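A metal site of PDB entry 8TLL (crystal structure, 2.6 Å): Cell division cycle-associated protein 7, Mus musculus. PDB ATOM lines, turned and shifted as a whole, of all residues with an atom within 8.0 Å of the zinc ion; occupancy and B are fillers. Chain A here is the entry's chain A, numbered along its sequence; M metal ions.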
ATOM      1  N   HIS A  10      10.333  -2.080  -7.937  1.00  0.00           N
ATOM      2  CA  HIS A  10      10.243  -3.072  -6.865  1.00  0.00           C
ATOM      3  C   HIS A  10      11.471  -3.967  -6.913  1.00  0.00           C
ATOM      4  O   HIS A  10      11.734  -4.629  -7.924  1.00  0.00           O
ATOM      5  CB  HIS A  10       8.957  -3.893  -6.992  1.00  0.00           C
ATOM      6  CG  HIS A  10       8.951  -5.116  -6.128  1.00  0.00           C
ATOM      7  ND1 HIS A  10       8.656  -6.368  -6.616  1.00  0.00           N
ATOM      8  CD2 HIS A  10       9.217  -5.281  -4.810  1.00  0.00           C
ATOM      9  CE1 HIS A  10       8.738  -7.253  -5.642  1.00  0.00           C
ATOM     10  NE2 HIS A  10       9.076  -6.617  -4.536  1.00  0.00           N
ATOM     11  N   ASN A  56       8.861  -5.881   2.452  1.00  0.00           N
ATOM     12  CA  ASN A  56       9.269  -6.029   1.069  1.00  0.00           C
ATOM     13  C   ASN A  56       8.611  -7.272   0.494  1.00  0.00           C
ATOM     14  O   ASN A  56       8.848  -8.381   0.974  1.00  0.00           O
ATOM     15  CB  ASN A  56      10.800  -6.122   0.960  1.00  0.00           C
ATOM     16  CG  ASN A  56      11.276  -6.311  -0.467  1.00  0.00           C
ATOM     17  OD1 ASN A  56      11.740  -7.386  -0.841  1.00  0.00           O
ATOM     18  ND2 ASN A  56      11.163  -5.249  -1.266  1.00  0.00           N
ATOM     19  N   CYS A  57       7.768  -7.085  -0.525  1.00  0.00           N
ATOM     20  CA  CYS A  57       7.073  -8.209  -1.128  1.00  0.00           C
ATOM     21  C   CYS A  57       8.048  -9.046  -1.951  1.00  0.00           C
ATOM     22  O   CYS A  57       8.906  -8.517  -2.654  1.00  0.00           O
ATOM     23  CB  CYS A  57       5.924  -7.711  -2.007  1.00  0.00           C
ATOM     24  SG  CYS A  57       4.805  -9.006  -2.632  1.00  0.00           S
ATOM     25  N   ARG A  58       7.903 -10.377  -1.860  1.00  0.00           N
ATOM     26  CA  ARG A  58       8.747 -11.310  -2.592  1.00  0.00           C
ATOM     27  C   ARG A  58       8.093 -11.846  -3.860  1.00  0.00           C
ATOM     28  O   ARG A  58       8.683 -12.713  -4.522  1.00  0.00           O
ATOM     29  CB  ARG A  58       9.143 -12.488  -1.687  1.00  0.00           C
ATOM     30  CG  ARG A  58      10.486 -12.325  -0.998  1.00  0.00           C
ATOM     31  CD  ARG A  58      10.385 -11.443   0.228  1.00  0.00           C
ATOM     32  NE  ARG A  58      11.678 -11.246   0.866  1.00  0.00           N
ATOM     33  CZ  ARG A  58      11.851 -10.667   2.050  1.00  0.00           C
ATOM     34  NH1 ARG A  58      10.817 -10.248   2.764  1.00  0.00           N
ATOM     35  NH2 ARG A  58      13.081 -10.502   2.525  1.00  0.00           N
ATOM     36  N   ASN A  59       6.902 -11.393  -4.204  1.00  0.00           N
ATOM     37  CA  ASN A  59       6.256 -11.853  -5.428  1.00  0.00           C
ATOM     38  C   ASN A  59       6.948 -11.245  -6.637  1.00  0.00           C
ATOM     39  O   ASN A  59       7.033 -10.014  -6.732  1.00  0.00           O
ATOM     40  CB  ASN A  59       4.772 -11.472  -5.407  1.00  0.00           C
ATOM     41  CG  ASN A  59       4.021 -11.964  -6.635  1.00  0.00           C
ATOM     42  OD1 ASN A  59       4.416 -12.939  -7.277  1.00  0.00           O
ATOM     43  ND2 ASN A  59       2.938 -11.279  -6.979  1.00  0.00           N
ATOM     44  N   PRO A  60       7.465 -12.055  -7.569  1.00  0.00           N
ATOM     45  CA  PRO A  60       8.147 -11.460  -8.746  1.00  0.00           C
ATOM     46  C   PRO A  60       7.252 -10.548  -9.561  1.00  0.00           C
ATOM     47  O   PRO A  60       7.724  -9.523 -10.071  1.00  0.00           O
ATOM     48  CB  PRO A  60       8.591 -12.693  -9.540  1.00  0.00           C
ATOM     49  CG  PRO A  60       8.665 -13.798  -8.543  1.00  0.00           C
ATOM     50  CD  PRO A  60       7.566 -13.522  -7.559  1.00  0.00           C
ATOM     51  N   ASP A  61       5.966 -10.872  -9.708  1.00  0.00           N
ATOM     52  CA  ASP A  61       5.069 -10.066 -10.518  1.00  0.00           C
ATOM     53  C   ASP A  61       4.557  -8.840  -9.772  1.00  0.00           C
ATOM     54  O   ASP A  61       3.902  -7.992 -10.390  1.00  0.00           O
ATOM     55  CB  ASP A  61       3.887 -10.904 -11.010  1.00  0.00           C
ATOM     56  CG  ASP A  61       3.126 -10.224 -12.145  1.00  0.00           C
ATOM     57  OD1 ASP A  61       3.726 -10.015 -13.222  1.00  0.00           O
ATOM     58  OD2 ASP A  61       1.932  -9.911 -11.966  1.00  0.00           O
ATOM     59  N   CYS A  62       4.831  -8.722  -8.474  1.00  0.00           N
ATOM     60  CA  CYS A  62       4.460  -7.523  -7.735  1.00  0.00           C
ATOM     61  C   CYS A  62       5.257  -6.324  -8.256  1.00  0.00           C
ATOM     62  O   CYS A  62       6.310  -6.470  -8.890  1.00  0.00           O
ATOM     63  CB  CYS A  62       4.705  -7.713  -6.241  1.00  0.00           C
ATOM     64  SG  CYS A  62       3.974  -6.459  -5.139  1.00  0.00           S
ATOM     65  N   TRP A  63       4.730  -5.134  -8.007  1.00  0.00           N
ATOM     66  CA  TRP A  63       5.316  -3.921  -8.540  1.00  0.00           C
ATOM     67  C   TRP A  63       5.012  -2.755  -7.621  1.00  0.00           C
ATOM     68  O   TRP A  63       4.089  -2.811  -6.805  1.00  0.00           O
ATOM     69  CB  TRP A  63       4.794  -3.621  -9.948  1.00  0.00           C
ATOM     70  CG  TRP A  63       3.398  -3.063  -9.935  1.00  0.00           C
ATOM     71  CD1 TRP A  63       3.030  -1.753  -9.975  1.00  0.00           C
ATOM     72  CD2 TRP A  63       2.179  -3.819  -9.848  1.00  0.00           C
ATOM     73  NE1 TRP A  63       1.654  -1.639  -9.934  1.00  0.00           N
ATOM     74  CE2 TRP A  63       1.116  -2.896  -9.860  1.00  0.00           C
ATOM     75  CE3 TRP A  63       1.877  -5.184  -9.770  1.00  0.00           C
ATOM     76  CZ2 TRP A  63      -0.222  -3.291  -9.786  1.00  0.00           C
ATOM     77  CZ3 TRP A  63       0.558  -5.573  -9.710  1.00  0.00           C
ATOM     78  CH2 TRP A  63      -0.473  -4.625  -9.716  1.00  0.00           C
ATOM     79  N   GLY A  64       5.785  -1.683  -7.776  1.00  0.00           N
ATOM     80  CA  GLY A  64       5.453  -0.422  -7.133  1.00  0.00           C
ATOM     81  C   GLY A  64       5.605  -0.467  -5.627  1.00  0.00           C
ATOM     82  O   GLY A  64       6.480  -1.151  -5.082  1.00  0.00           O
ATOM     83  N   ILE A  65       4.725   0.250  -4.938  1.00  0.00           N
ATOM     84  CA  ILE A  65       4.855   0.500  -3.506  1.00  0.00           C
ATOM     85  C   ILE A  65       3.866  -0.304  -2.669  1.00  0.00           C
ATOM     86  O   ILE A  65       3.986  -0.312  -1.430  1.00  0.00           O
ATOM     87  CB  ILE A  65       4.710   2.013  -3.191  1.00  0.00           C
ATOM     88  CG1 ILE A  65       5.792   2.457  -2.219  1.00  0.00           C
ATOM     89  CG2 ILE A  65       3.312   2.360  -2.689  1.00  0.00           C
ATOM     90  CD1 ILE A  65       7.180   2.406  -2.809  1.00  0.00           C
ATOM     91  N   ARG A  66       2.937  -1.028  -3.295  1.00  0.00           N
ATOM     92  CA  ARG A  66       1.845  -1.670  -2.585  1.00  0.00           C
ATOM     93  C   ARG A  66       2.298  -2.804  -1.668  1.00  0.00           C
ATOM     94  O   ARG A  66       1.481  -3.290  -0.879  1.00  0.00           O
ATOM     95  CB  ARG A  66       0.816  -2.197  -3.580  1.00  0.00           C
ATOM     96  CG  ARG A  66       1.437  -2.767  -4.846  1.00  0.00           C
ATOM     97  CD  ARG A  66       0.385  -3.416  -5.711  1.00  0.00           C
ATOM     98  NE  ARG A  66       0.481  -4.870  -5.658  1.00  0.00           N
ATOM     99  CZ  ARG A  66      -0.422  -5.699  -6.171  1.00  0.00           C
ATOM    100  NH1 ARG A  66      -1.520  -5.242  -6.755  1.00  0.00           N
ATOM    101  NH2 ARG A  66      -0.212  -7.001  -6.091  1.00  0.00           N
ATOM    102  N   GLY A  67       3.554  -3.239  -1.762  1.00  0.00           N
ATOM    103  CA  GLY A  67       4.084  -4.231  -0.853  1.00  0.00           C
ATOM    104  C   GLY A  67       4.723  -3.693   0.407  1.00  0.00           C
ATOM    105  O   GLY A  67       5.238  -4.467   1.206  1.00  0.00           O
ATOM    106  N   GLN A  68       4.711  -2.374   0.608  1.00  0.00           N
ATOM    107  CA  GLN A  68       5.391  -1.752   1.732  1.00  0.00           C
ATOM    108  C   GLN A  68       4.383  -1.394   2.816  1.00  0.00           C
ATOM    109  O   GLN A  68       3.482  -0.596   2.576  1.00  0.00           O
ATOM    110  CB  GLN A  68       6.158  -0.502   1.301  1.00  0.00           C
ATOM    111  CG  GLN A  68       7.333  -0.760   0.405  1.00  0.00           C
ATOM    112  CD  GLN A  68       7.981   0.537  -0.033  1.00  0.00           C
ATOM    113  OE1 GLN A  68       7.532   1.610   0.348  1.00  0.00           O
ATOM    114  NE2 GLN A  68       9.026   0.432  -0.848  1.00  0.00           N
ATOM    115  N   PHE A  69       4.571  -1.961   3.998  1.00  0.00           N
ATOM    116  CA  PHE A  69       3.691  -1.732   5.134  1.00  0.00           C
ATOM    117  C   PHE A  69       4.535  -1.355   6.340  1.00  0.00           C
ATOM    118  O   PHE A  69       5.598  -1.942   6.569  1.00  0.00           O
ATOM    119  CB  PHE A  69       2.851  -2.978   5.447  1.00  0.00           C
ATOM    120  CG  PHE A  69       1.760  -3.229   4.444  1.00  0.00           C
ATOM    121  CD1 PHE A  69       2.034  -3.830   3.229  1.00  0.00           C
ATOM    122  CD2 PHE A  69       0.454  -2.858   4.728  1.00  0.00           C
ATOM    123  CE1 PHE A  69       1.033  -4.064   2.313  1.00  0.00           C
ATOM    124  CE2 PHE A  69      -0.561  -3.090   3.813  1.00  0.00           C
ATOM    125  CZ  PHE A  69      -0.264  -3.686   2.605  1.00  0.00           C
ATOM    126  N   TRP A  91       6.975 -14.531   1.681  1.00  0.00           N
ATOM    127  CA  TRP A  91       5.957 -13.573   2.090  1.00  0.00           C
ATOM    128  C   TRP A  91       5.456 -12.776   0.892  1.00  0.00           C
ATOM    129  O   TRP A  91       6.250 -12.210   0.132  1.00  0.00           O
ATOM    130  CB  TRP A  91       6.505 -12.645   3.169  1.00  0.00           C
ATOM    131  CG  TRP A  91       5.470 -11.747   3.752  1.00  0.00           C
ATOM    132  CD1 TRP A  91       4.625 -12.030   4.788  1.00  0.00           C
ATOM    133  CD2 TRP A  91       5.168 -10.406   3.345  1.00  0.00           C
ATOM    134  NE1 TRP A  91       3.815 -10.954   5.053  1.00  0.00           N
ATOM    135  CE2 TRP A  91       4.125  -9.939   4.185  1.00  0.00           C
ATOM    136  CE3 TRP A  91       5.666  -9.557   2.366  1.00  0.00           C
ATOM    137  CZ2 TRP A  91       3.579  -8.667   4.054  1.00  0.00           C
ATOM    138  CZ3 TRP A  91       5.127  -8.292   2.243  1.00  0.00           C
ATOM    139  CH2 TRP A  91       4.088  -7.861   3.081  1.00  0.00           C
ATOM    140  N   HIS A  92       4.137 -12.734   0.727  1.00  0.00           N
ATOM    141  CA  HIS A  92       3.469 -11.904  -0.256  1.00  0.00           C
ATOM    142  C   HIS A  92       2.659 -10.839   0.476  1.00  0.00           C
ATOM    143  O   HIS A  92       2.085 -11.114   1.535  1.00  0.00           O
ATOM    144  CB  HIS A  92       2.550 -12.721  -1.172  1.00  0.00           C
ATOM    145  CG  HIS A  92       3.275 -13.637  -2.095  1.00  0.00           C
ATOM    146  ND1 HIS A  92       4.646 -13.744  -2.125  1.00  0.00           N
ATOM    147  CD2 HIS A  92       2.810 -14.513  -3.025  1.00  0.00           C
ATOM    148  CE1 HIS A  92       5.000 -14.638  -3.031  1.00  0.00           C
ATOM    149  NE2 HIS A  92       3.904 -15.119  -3.595  1.00  0.00           N
ATOM    150  N   CYS A  93       2.608  -9.640  -0.094  1.00  0.00           N
ATOM    151  CA  CYS A  93       1.876  -8.574   0.552  1.00  0.00           C
ATOM    152  C   CYS A  93       0.376  -8.858   0.518  1.00  0.00           C
ATOM    153  O   CYS A  93      -0.087  -9.696  -0.268  1.00  0.00           O
ATOM    154  CB  CYS A  93       2.189  -7.231  -0.118  1.00  0.00           C
ATOM    155  SG  CYS A  93       1.675  -7.088  -1.830  1.00  0.00           S
ATOM    156  N   PRO A  94      -0.398  -8.235   1.397  1.00  0.00           N
ATOM    157  CA  PRO A  94      -1.845  -8.433   1.407  1.00  0.00           C
ATOM    158  C   PRO A  94      -2.491  -8.115   0.063  1.00  0.00           C
ATOM    159  O   PRO A  94      -3.445  -8.800  -0.333  1.00  0.00           O
ATOM    160  CB  PRO A  94      -2.324  -7.467   2.501  1.00  0.00           C
ATOM    161  CG  PRO A  94      -1.174  -7.362   3.426  1.00  0.00           C
ATOM    162  CD  PRO A  94       0.066  -7.486   2.586  1.00  0.00           C
ATOM    163  N   PRO A  95      -2.033  -7.083  -0.678  1.00  0.00           N
ATOM    164  CA  PRO A  95      -2.559  -6.926  -2.041  1.00  0.00           C
ATOM    165  C   PRO A  95      -2.348  -8.147  -2.925  1.00  0.00           C
ATOM    166  O   PRO A  95      -3.245  -8.509  -3.683  1.00  0.00           O
ATOM    167  CB  PRO A  95      -1.789  -5.710  -2.556  1.00  0.00           C
ATOM    168  CG  PRO A  95      -1.568  -4.902  -1.351  1.00  0.00           C
ATOM    169  CD  PRO A  95      -1.280  -5.888  -0.265  1.00  0.00           C
ATOM    170  N   CYS A  96      -1.179  -8.791  -2.839  1.00  0.00           N
ATOM    171  CA  CYS A  96      -0.960 -10.017  -3.603  1.00  0.00           C
ATOM    172  C   CYS A  96      -1.842 -11.150  -3.105  1.00  0.00           C
ATOM    173  O   CYS A  96      -2.390 -11.922  -3.913  1.00  0.00           O
ATOM    174  CB  CYS A  96       0.515 -10.420  -3.542  1.00  0.00           C
ATOM    175  SG  CYS A  96       1.631  -9.460  -4.598  1.00  0.00           S
ATOM    176  N   ARG A  97      -2.000 -11.281  -1.790  1.00  0.00           N
ATOM    177  CA  ARG A  97      -2.928 -12.254  -1.235  1.00  0.00           C
ATOM    178  C   ARG A  97      -4.378 -11.878  -1.455  1.00  0.00           C
ATOM    179  O   ARG A  97      -5.263 -12.706  -1.207  1.00  0.00           O
ATOM    180  CB  ARG A  97      -2.662 -12.439   0.255  1.00  0.00           C
ATOM    181  CG  ARG A  97      -1.426 -13.265   0.564  1.00  0.00           C
ATOM    182  CD  ARG A  97      -1.196 -13.375   2.054  1.00  0.00           C
ATOM    183  NE  ARG A  97      -0.630 -12.137   2.604  1.00  0.00           N
ATOM    184  CZ  ARG A  97      -0.239 -11.994   3.862  1.00  0.00           C
ATOM    185  NH1 ARG A  97      -0.356 -12.970   4.737  1.00  0.00           N
ATOM    186  NH2 ARG A  97       0.281 -10.839   4.244  1.00  0.00           N
HETATM  187 ZN    ZN M   1       2.968  -7.843  -3.510  1.00  0.00          ZN
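The backbone carbonyl oxygen of Cys 57 sits at hydrogen-bond distance from a ring nitrogen (NE2) of His 10 (2.7 Å). SG of Cys 96 lies close to NH2 of Arg 66. SG of Cys 57 sits close to N of Asn 59. ND2 of Asn 59 sits close to SG of Cys 96 (3.3 Å). O of Cys 62 is in hydrogen-bond range of ND1 of His 10 (3.3 Å).
Of the 22 residues printed, 4 come within 4 Å of the zinc ion. The nearest printed residue that does not touch the zinc ion is Arg 66 (4.2 Å).
SG of Cys 93 binds the zinc ion (2.3 Å). SG of Cys 57 binds the zinc ion (2.3 Å). The zinc ion is bound by the side-chain sulfur (SG) of Cys 62 (2.4 Å). SG of Cys 96 binds the zinc ion, 2.4 Å away.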
